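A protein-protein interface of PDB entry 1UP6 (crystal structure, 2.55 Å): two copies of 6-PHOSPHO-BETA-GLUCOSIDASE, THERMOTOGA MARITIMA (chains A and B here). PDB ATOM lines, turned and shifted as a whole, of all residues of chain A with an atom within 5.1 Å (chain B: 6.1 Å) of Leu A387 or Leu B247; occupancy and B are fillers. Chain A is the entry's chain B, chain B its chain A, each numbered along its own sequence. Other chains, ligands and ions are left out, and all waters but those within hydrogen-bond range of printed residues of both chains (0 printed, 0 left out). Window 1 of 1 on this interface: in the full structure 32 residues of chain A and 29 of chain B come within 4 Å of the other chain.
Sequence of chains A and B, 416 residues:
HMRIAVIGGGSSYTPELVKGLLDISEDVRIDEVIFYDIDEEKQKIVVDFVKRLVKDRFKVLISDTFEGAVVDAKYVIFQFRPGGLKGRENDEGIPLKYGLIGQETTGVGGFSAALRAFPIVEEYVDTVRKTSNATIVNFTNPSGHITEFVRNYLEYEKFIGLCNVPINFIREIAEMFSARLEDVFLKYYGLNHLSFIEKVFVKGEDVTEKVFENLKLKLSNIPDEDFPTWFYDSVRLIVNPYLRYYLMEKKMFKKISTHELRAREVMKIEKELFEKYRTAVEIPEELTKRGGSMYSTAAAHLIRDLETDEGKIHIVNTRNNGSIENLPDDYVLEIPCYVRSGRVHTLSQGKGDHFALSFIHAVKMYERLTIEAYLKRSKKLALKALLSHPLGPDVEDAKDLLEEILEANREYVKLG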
ATOM      1  N   ALA A 382       6.880  31.647  32.947  1.00  0.00           N
ATOM      2  CA  ALA A 382       5.924  32.722  32.606  1.00  0.00           C
ATOM      3  C   ALA A 382       5.702  32.818  31.111  1.00  0.00           C
ATOM      4  O   ALA A 382       4.583  33.043  30.653  1.00  0.00           O
ATOM      5  CB  ALA A 382       6.360  34.067  33.188  1.00  0.00           C
ATOM      6  N   LEU A 383       6.786  32.611  30.368  1.00  0.00           N
ATOM      7  CA  LEU A 383       6.791  32.526  28.907  1.00  0.00           C
ATOM      8  C   LEU A 383       5.909  31.372  28.432  1.00  0.00           C
ATOM      9  O   LEU A 383       5.095  31.535  27.523  1.00  0.00           O
ATOM     10  CB  LEU A 383       8.223  32.278  28.449  1.00  0.00           C
ATOM     11  CG  LEU A 383       8.995  33.367  27.681  1.00  0.00           C
ATOM     12  CD1 LEU A 383       8.236  34.668  27.621  1.00  0.00           C
ATOM     13  CD2 LEU A 383      10.359  33.626  28.280  1.00  0.00           C
ATOM     14  N   LYS A 384       6.094  30.219  29.073  1.00  0.00           N
ATOM     15  CA  LYS A 384       5.298  29.038  28.842  1.00  0.00           C
ATOM     16  C   LYS A 384       3.792  29.317  29.085  1.00  0.00           C
ATOM     17  O   LYS A 384       2.958  28.964  28.263  1.00  0.00           O
ATOM     18  CB  LYS A 384       5.840  27.911  29.759  1.00  0.00           C
ATOM     19  CG  LYS A 384       5.333  26.553  29.451  1.00  0.00           C
ATOM     20  CD  LYS A 384       6.046  25.518  30.273  1.00  0.00           C
ATOM     21  CE  LYS A 384       5.178  24.288  30.428  1.00  0.00           C
ATOM     22  NZ  LYS A 384       5.915  23.016  30.694  1.00  0.00           N
ATOM     23  N   ALA A 385       3.469  29.970  30.197  1.00  0.00           N
ATOM     24  CA  ALA A 385       2.091  30.345  30.511  1.00  0.00           C
ATOM     25  C   ALA A 385       1.489  31.283  29.443  1.00  0.00           C
ATOM     26  O   ALA A 385       0.369  31.068  28.963  1.00  0.00           O
ATOM     27  CB  ALA A 385       2.011  30.961  31.899  1.00  0.00           C
ATOM     28  N   LEU A 386       2.268  32.283  29.055  1.00  0.00           N
ATOM     29  CA  LEU A 386       1.845  33.277  28.057  1.00  0.00           C
ATOM     30  C   LEU A 386       1.548  32.687  26.697  1.00  0.00           C
ATOM     31  O   LEU A 386       0.549  33.043  26.041  1.00  0.00           O
ATOM     32  CB  LEU A 386       2.937  34.325  27.916  1.00  0.00           C
ATOM     33  CG  LEU A 386       2.683  35.825  27.799  1.00  0.00           C
ATOM     34  CD1 LEU A 386       1.394  36.335  28.377  1.00  0.00           C
ATOM     35  CD2 LEU A 386       3.887  36.522  28.460  1.00  0.00           C
ATOM     36  N   LEU A 387       2.420  31.770  26.280  1.00  0.00           N
ATOM     37  CA  LEU A 387       2.237  31.062  25.014  1.00  0.00           C
ATOM     38  C   LEU A 387       1.045  30.118  24.975  1.00  0.00           C
ATOM     39  O   LEU A 387       0.588  29.794  23.903  1.00  0.00           O
ATOM     40  CB  LEU A 387       3.506  30.309  24.655  1.00  0.00           C
ATOM     41  CG  LEU A 387       4.669  31.208  24.250  1.00  0.00           C
ATOM     42  CD1 LEU A 387       5.923  30.373  24.333  1.00  0.00           C
ATOM     43  CD2 LEU A 387       4.475  31.773  22.853  1.00  0.00           C
ATOM     44  N   SER A 388       0.555  29.693  26.135  1.00  0.00           N
ATOM     45  CA  SER A 388      -0.541  28.746  26.236  1.00  0.00           C
ATOM     46  C   SER A 388      -1.918  29.406  26.116  1.00  0.00           C
ATOM     47  O   SER A 388      -2.890  28.724  25.768  1.00  0.00           O
ATOM     48  CB  SER A 388      -0.431  27.961  27.556  1.00  0.00           C
ATOM     49  OG  SER A 388      -0.888  28.714  28.696  1.00  0.00           O
ATOM     50  N   HIS A 389      -2.015  30.704  26.407  1.00  0.00           N
ATOM     51  CA  HIS A 389      -3.299  31.398  26.325  1.00  0.00           C
ATOM     52  C   HIS A 389      -3.816  31.485  24.882  1.00  0.00           C
ATOM     53  O   HIS A 389      -3.077  31.891  24.020  1.00  0.00           O
ATOM     54  CB  HIS A 389      -3.257  32.807  26.960  1.00  0.00           C
ATOM     55  CG  HIS A 389      -4.616  33.291  27.356  1.00  0.00           C
ATOM     56  ND1 HIS A 389      -5.557  33.688  26.429  1.00  0.00           N
ATOM     57  CD2 HIS A 389      -5.233  33.331  28.561  1.00  0.00           C
ATOM     58  CE1 HIS A 389      -6.685  33.991  27.050  1.00  0.00           C
ATOM     59  NE2 HIS A 389      -6.516  33.777  28.344  1.00  0.00           N
ATOM     60  N   PRO A 393       0.490  35.726  22.940  1.00  0.00           N
ATOM     61  CA  PRO A 393       1.393  36.082  21.829  1.00  0.00           C
ATOM     62  C   PRO A 393       1.948  34.900  21.075  1.00  0.00           C
ATOM     63  O   PRO A 393       2.040  33.801  21.578  1.00  0.00           O
ATOM     64  CB  PRO A 393       2.533  36.837  22.534  1.00  0.00           C
ATOM     65  CG  PRO A 393       2.560  36.232  23.962  1.00  0.00           C
ATOM     66  CD  PRO A 393       1.114  35.907  24.266  1.00  0.00           C
ATOM     67  N   ASP A 394       2.271  35.146  19.822  1.00  0.00           N
ATOM     68  CA  ASP A 394       3.046  34.240  19.009  1.00  0.00           C
ATOM     69  C   ASP A 394       4.478  34.172  19.604  1.00  0.00           C
ATOM     70  O   ASP A 394       4.945  35.083  20.284  1.00  0.00           O
ATOM     71  CB  ASP A 394       3.145  34.838  17.600  1.00  0.00           C
ATOM     72  CG  ASP A 394       2.070  34.357  16.647  1.00  0.00           C
ATOM     73  OD1 ASP A 394       1.073  33.694  17.063  1.00  0.00           O
ATOM     74  OD2 ASP A 394       2.167  34.594  15.425  1.00  0.00           O
ATOM     75  N   VAL A 395       5.196  33.098  19.317  1.00  0.00           N
ATOM     76  CA  VAL A 395       6.586  32.956  19.756  1.00  0.00           C
ATOM     77  C   VAL A 395       7.445  34.201  19.434  1.00  0.00           C
ATOM     78  O   VAL A 395       8.257  34.630  20.265  1.00  0.00           O
ATOM     79  CB  VAL A 395       7.216  31.672  19.152  1.00  0.00           C
ATOM     80  CG1 VAL A 395       8.724  31.633  19.334  1.00  0.00           C
ATOM     81  CG2 VAL A 395       6.580  30.435  19.789  1.00  0.00           C
ATOM     82  N   ALA A 398       6.775  36.991  22.223  1.00  0.00           N
ATOM     83  CA  ALA A 398       6.647  36.628  23.641  1.00  0.00           C
ATOM     84  C   ALA A 398       7.743  37.235  24.588  1.00  0.00           C
ATOM     85  O   ALA A 398       7.444  37.729  25.703  1.00  0.00           O
ATOM     86  CB  ALA A 398       6.583  35.129  23.795  1.00  0.00           C
ATOM     87  N   PHE B 227      11.670  26.962  16.231  1.00  0.00           N
ATOM     88  CA  PHE B 227      11.559  27.465  17.576  1.00  0.00           C
ATOM     89  C   PHE B 227      12.902  27.947  17.997  1.00  0.00           C
ATOM     90  O   PHE B 227      13.881  27.267  17.746  1.00  0.00           O
ATOM     91  CB  PHE B 227      11.020  26.367  18.472  1.00  0.00           C
ATOM     92  CG  PHE B 227       9.638  25.958  18.101  1.00  0.00           C
ATOM     93  CD1 PHE B 227       8.549  26.761  18.436  1.00  0.00           C
ATOM     94  CD2 PHE B 227       9.424  24.816  17.355  1.00  0.00           C
ATOM     95  CE1 PHE B 227       7.275  26.404  18.078  1.00  0.00           C
ATOM     96  CE2 PHE B 227       8.123  24.442  16.978  1.00  0.00           C
ATOM     97  CZ  PHE B 227       7.056  25.228  17.359  1.00  0.00           C
ATOM     98  N   TRP B 230      15.368  29.793  23.581  1.00  0.00           N
ATOM     99  CA  TRP B 230      14.634  30.089  24.806  1.00  0.00           C
ATOM    100  C   TRP B 230      13.311  29.306  24.914  1.00  0.00           C
ATOM    101  O   TRP B 230      12.881  29.001  26.030  1.00  0.00           O
ATOM    102  CB  TRP B 230      14.432  31.593  24.961  1.00  0.00           C
ATOM    103  CG  TRP B 230      13.516  32.228  23.941  1.00  0.00           C
ATOM    104  CD1 TRP B 230      13.890  32.984  22.860  1.00  0.00           C
ATOM    105  CD2 TRP B 230      12.083  32.183  23.924  1.00  0.00           C
ATOM    106  NE1 TRP B 230      12.773  33.396  22.170  1.00  0.00           N
ATOM    107  CE2 TRP B 230      11.652  32.925  22.804  1.00  0.00           C
ATOM    108  CE3 TRP B 230      11.119  31.600  24.746  1.00  0.00           C
ATOM    109  CZ2 TRP B 230      10.311  33.099  22.489  1.00  0.00           C
ATOM    110  CZ3 TRP B 230       9.758  31.747  24.404  1.00  0.00           C
ATOM    111  CH2 TRP B 230       9.380  32.496  23.294  1.00  0.00           C
ATOM    112  N   PHE B 231      12.714  28.945  23.772  1.00  0.00           N
ATOM    113  CA  PHE B 231      11.471  28.169  23.747  1.00  0.00           C
ATOM    114  C   PHE B 231      11.618  26.820  24.442  1.00  0.00           C
ATOM    115  O   PHE B 231      10.791  26.445  25.273  1.00  0.00           O
ATOM    116  CB  PHE B 231      10.992  27.981  22.316  1.00  0.00           C
ATOM    117  CG  PHE B 231       9.692  27.227  22.188  1.00  0.00           C
ATOM    118  CD1 PHE B 231       8.468  27.889  22.316  1.00  0.00           C
ATOM    119  CD2 PHE B 231       9.699  25.865  21.883  1.00  0.00           C
ATOM    120  CE1 PHE B 231       7.283  27.197  22.156  1.00  0.00           C
ATOM    121  CE2 PHE B 231       8.519  25.172  21.731  1.00  0.00           C
ATOM    122  CZ  PHE B 231       7.305  25.829  21.858  1.00  0.00           C
ATOM    123  N   SER B 234      12.012  27.146  28.062  1.00  0.00           N
ATOM    124  CA  SER B 234      10.785  27.553  28.749  1.00  0.00           C
ATOM    125  C   SER B 234       9.794  26.438  28.873  1.00  0.00           C
ATOM    126  O   SER B 234       9.256  26.193  29.936  1.00  0.00           O
ATOM    127  CB  SER B 234      10.124  28.702  28.001  1.00  0.00           C
ATOM    128  OG  SER B 234      10.752  29.885  28.438  1.00  0.00           O
ATOM    129  N   VAL B 235       9.556  25.786  27.753  1.00  0.00           N
ATOM    130  CA  VAL B 235       8.474  24.861  27.595  1.00  0.00           C
ATOM    131  C   VAL B 235       8.928  23.498  28.099  1.00  0.00           C
ATOM    132  O   VAL B 235       8.141  22.742  28.663  1.00  0.00           O
ATOM    133  CB  VAL B 235       8.072  24.842  26.104  1.00  0.00           C
ATOM    134  CG1 VAL B 235       7.180  23.680  25.771  1.00  0.00           C
ATOM    135  CG2 VAL B 235       7.436  26.214  25.724  1.00  0.00           C
ATOM    136  N   VAL B 239       8.763  19.505  20.683  1.00  0.00           N
ATOM    137  CA  VAL B 239       7.448  19.733  20.134  1.00  0.00           C
ATOM    138  C   VAL B 239       7.421  19.238  18.682  1.00  0.00           C
ATOM    139  O   VAL B 239       8.415  19.276  17.983  1.00  0.00           O
ATOM    140  CB  VAL B 239       7.138  21.246  20.295  1.00  0.00           C
ATOM    141  CG1 VAL B 239       7.241  21.995  19.005  1.00  0.00           C
ATOM    142  CG2 VAL B 239       5.812  21.478  20.953  1.00  0.00           C
ATOM    143  N   LEU B 243       3.464  22.075  15.309  1.00  0.00           N
ATOM    144  CA  LEU B 243       3.073  23.055  16.316  1.00  0.00           C
ATOM    145  C   LEU B 243       3.360  24.476  15.894  1.00  0.00           C
ATOM    146  O   LEU B 243       2.752  25.401  16.396  1.00  0.00           O
ATOM    147  CB  LEU B 243       3.703  22.791  17.676  1.00  0.00           C
ATOM    148  CG  LEU B 243       2.754  22.144  18.715  1.00  0.00           C
ATOM    149  CD1 LEU B 243       1.525  22.976  19.046  1.00  0.00           C
ATOM    150  CD2 LEU B 243       2.302  20.725  18.273  1.00  0.00           C
ATOM    151  N   ARG B 244       4.279  24.637  14.952  1.00  0.00           N
ATOM    152  CA  ARG B 244       4.562  25.934  14.358  1.00  0.00           C
ATOM    153  C   ARG B 244       3.313  26.660  13.846  1.00  0.00           C
ATOM    154  O   ARG B 244       3.245  27.871  13.973  1.00  0.00           O
ATOM    155  CB  ARG B 244       5.541  25.781  13.193  1.00  0.00           C
ATOM    156  CG  ARG B 244       6.990  25.911  13.595  1.00  0.00           C
ATOM    157  CD  ARG B 244       7.912  24.946  12.861  1.00  0.00           C
ATOM    158  NE  ARG B 244       8.165  25.340  11.481  1.00  0.00           N
ATOM    159  CZ  ARG B 244       7.798  24.642  10.402  1.00  0.00           C
ATOM    160  NH1 ARG B 244       7.149  23.491  10.508  1.00  0.00           N
ATOM    161  NH2 ARG B 244       8.092  25.120   9.192  1.00  0.00           N
ATOM    162  N   TYR B 245       2.329  25.927  13.287  1.00  0.00           N
ATOM    163  CA  TYR B 245       1.130  26.582  12.759  1.00  0.00           C
ATOM    164  C   TYR B 245       0.320  27.194  13.905  1.00  0.00           C
ATOM    165  O   TYR B 245      -0.372  28.184  13.711  1.00  0.00           O
ATOM    166  CB  TYR B 245       0.289  25.607  11.902  1.00  0.00           C
ATOM    167  CG  TYR B 245       1.074  25.043  10.761  1.00  0.00           C
ATOM    168  CD1 TYR B 245       1.382  25.829   9.660  1.00  0.00           C
ATOM    169  CD2 TYR B 245       1.564  23.738  10.800  1.00  0.00           C
ATOM    170  CE1 TYR B 245       2.148  25.321   8.602  1.00  0.00           C
ATOM    171  CE2 TYR B 245       2.326  23.227   9.766  1.00  0.00           C
ATOM    172  CZ  TYR B 245       2.615  24.019   8.682  1.00  0.00           C
ATOM    173  OH  TYR B 245       3.378  23.527   7.650  1.00  0.00           O
ATOM    174  N   TYR B 246       0.432  26.603  15.101  1.00  0.00           N
ATOM    175  CA  TYR B 246      -0.244  27.115  16.293  1.00  0.00           C
ATOM    176  C   TYR B 246       0.555  28.266  16.895  1.00  0.00           C
ATOM    177  O   TYR B 246       0.064  29.377  16.978  1.00  0.00           O
ATOM    178  CB  TYR B 246      -0.504  25.998  17.322  1.00  0.00           C
ATOM    179  CG  TYR B 246      -1.492  24.959  16.847  1.00  0.00           C
ATOM    180  CD1 TYR B 246      -1.079  23.868  16.067  1.00  0.00           C
ATOM    181  CD2 TYR B 246      -2.856  25.082  17.139  1.00  0.00           C
ATOM    182  CE1 TYR B 246      -1.996  22.927  15.611  1.00  0.00           C
ATOM    183  CE2 TYR B 246      -3.779  24.138  16.688  1.00  0.00           C
ATOM    184  CZ  TYR B 246      -3.342  23.060  15.927  1.00  0.00           C
ATOM    185  OH  TYR B 246      -4.253  22.130  15.473  1.00  0.00           O
ATOM    186  N   LEU B 247       1.816  28.028  17.251  1.00  0.00           N
ATOM    187  CA  LEU B 247       2.595  28.955  18.070  1.00  0.00           C
ATOM    188  C   LEU B 247       3.306  30.055  17.280  1.00  0.00           C
ATOM    189  O   LEU B 247       3.758  31.079  17.847  1.00  0.00           O
ATOM    190  CB  LEU B 247       3.626  28.175  18.866  1.00  0.00           C
ATOM    191  CG  LEU B 247       3.336  27.579  20.260  1.00  0.00           C
ATOM    192  CD1 LEU B 247       2.016  28.034  20.891  1.00  0.00           C
ATOM    193  CD2 LEU B 247       3.443  26.090  20.204  1.00  0.00           C
ATOM    194  N   MET B 248       3.446  29.833  15.971  1.00  0.00           N
ATOM    195  CA  MET B 248       3.982  30.877  15.072  1.00  0.00           C
ATOM    196  C   MET B 248       3.019  31.169  13.917  1.00  0.00           C
ATOM    197  O   MET B 248       3.461  31.250  12.760  1.00  0.00           O
ATOM    198  CB  MET B 248       5.369  30.488  14.518  1.00  0.00           C
ATOM    199  CG  MET B 248       6.388  30.094  15.590  1.00  0.00           C
ATOM    200  SD  MET B 248       8.119  29.322  14.956  1.00  0.00           S
ATOM    201  CE  MET B 248       8.659  30.683  13.832  1.00  0.00           C
ATOM    202  N   GLU B 249       1.722  31.304  14.239  1.00  0.00           N
ATOM    203  CA  GLU B 249       0.660  31.475  13.234  1.00  0.00           C
ATOM    204  C   GLU B 249       0.994  32.544  12.192  1.00  0.00           C
ATOM    205  O   GLU B 249       0.924  32.264  10.996  1.00  0.00           O
ATOM    206  CB  GLU B 249      -0.718  31.763  13.847  1.00  0.00           C
ATOM    207  CG  GLU B 249      -1.846  31.589  12.846  1.00  0.00           C
ATOM    208  CD  GLU B 249      -3.215  31.667  13.461  1.00  0.00           C
ATOM    209  OE1 GLU B 249      -3.338  31.798  14.712  1.00  0.00           O
ATOM    210  OE2 GLU B 249      -4.188  31.592  12.677  1.00  0.00           O
ATOM    211  N   PHE B 355       0.782  22.483  29.416  1.00  0.00           N
ATOM    212  CA  PHE B 355       0.992  23.109  28.107  1.00  0.00           C
ATOM    213  C   PHE B 355       0.563  22.171  26.977  1.00  0.00           C
ATOM    214  O   PHE B 355      -0.214  22.561  26.114  1.00  0.00           O
ATOM    215  CB  PHE B 355       2.471  23.517  27.966  1.00  0.00           C
ATOM    216  CG  PHE B 355       2.791  24.317  26.702  1.00  0.00           C
ATOM    217  CD1 PHE B 355       2.716  25.710  26.712  1.00  0.00           C
ATOM    218  CD2 PHE B 355       3.208  23.665  25.526  1.00  0.00           C
ATOM    219  CE1 PHE B 355       3.010  26.455  25.581  1.00  0.00           C
ATOM    220  CE2 PHE B 355       3.515  24.385  24.381  1.00  0.00           C
ATOM    221  CZ  PHE B 355       3.412  25.795  24.403  1.00  0.00           C
ATOM    222  N   PHE B 359      -3.411  22.069  24.180  1.00  0.00           N
ATOM    223  CA  PHE B 359      -3.538  21.697  22.774  1.00  0.00           C
ATOM    224  C   PHE B 359      -4.381  20.478  22.540  1.00  0.00           C
ATOM    225  O   PHE B 359      -5.301  20.541  21.722  1.00  0.00           O
ATOM    226  CB  PHE B 359      -2.172  21.554  22.083  1.00  0.00           C
ATOM    227  CG  PHE B 359      -1.508  22.866  21.857  1.00  0.00           C
ATOM    228  CD1 PHE B 359      -1.969  23.726  20.864  1.00  0.00           C
ATOM    229  CD2 PHE B 359      -0.489  23.292  22.699  1.00  0.00           C
ATOM    230  CE1 PHE B 359      -1.420  24.978  20.701  1.00  0.00           C
ATOM    231  CE2 PHE B 359       0.086  24.557  22.521  1.00  0.00           C
ATOM    232  CZ  PHE B 359      -0.397  25.394  21.515  1.00  0.00           C
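No position is printed for both chains.
Among the printed residues, pairs that only touch across the chains: Leu A383 with Trp B230, Leu A383 with Ser B234, Lys A384 with Ser B234, Lys A384 with Phe B355, Leu A387 with Leu B247, Leu A387 with Phe B355, Ser A388 with Phe B355, Asp A394 with Leu B247, Asp A394 with Met B248, Asp A394 with Glu B249, Val A395 with Trp B230, Val A395 with Met B248 and Ala A398 with Trp B230.
O of Val B235 lies within hydrogen-bond range of NZ of Lys A384 (3.0 Å). The backbone NH of Val A395 is in hydrogen-bond range of the backbone carbonyl oxygen of Leu B247, 2.9 Å away.
Of the printed residues of chain B, Leu A387 touches Leu B247 and Phe B355. Of the printed residues of chain B, Val A395 touches Trp B230 (3.4 Å), Leu B247 (2.9 Å) and Met B248 (3.98 Å). Of the printed residues of chain A, Trp B230 touches Leu A383, Val A395 and Ala A398. Leu B247 touches just these residues of chain A: Leu A387 (3.8 Å), Asp A394 (3.4 Å) and Val A395 (2.9 Å). The nearest printed residue of chain A that does not touch Glu B249 is Val A395 (6.4 Å).
O of Ala A385 is in hydrogen-bond range of OG of Ser A388 (2.7 Å). The backbone carbonyl oxygen of Trp B230 sits at hydrogen-bond distance from the side-chain hydroxyl of Ser B234 (3.3 Å).
Of the 12 printed residues of chain A, 7 touch a printed residue of chain B. Printed residues of chain B that touch a printed residue of chain A: Trp B230, Ser B234, Val B235, Leu B247, Met B248, Glu B249 and Phe B355. Hydrophobic or aromatic side chains of chain B that line the printed part of chain A: Trp B230, Leu B247, Met B248 and Phe B355. Among the printed residues, 15 pairs touch across the chains. Among the printed residues, no Asp or Glu carboxylate lies within 4 Å of a Lys or Arg side-chain nitrogen of the other chain.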
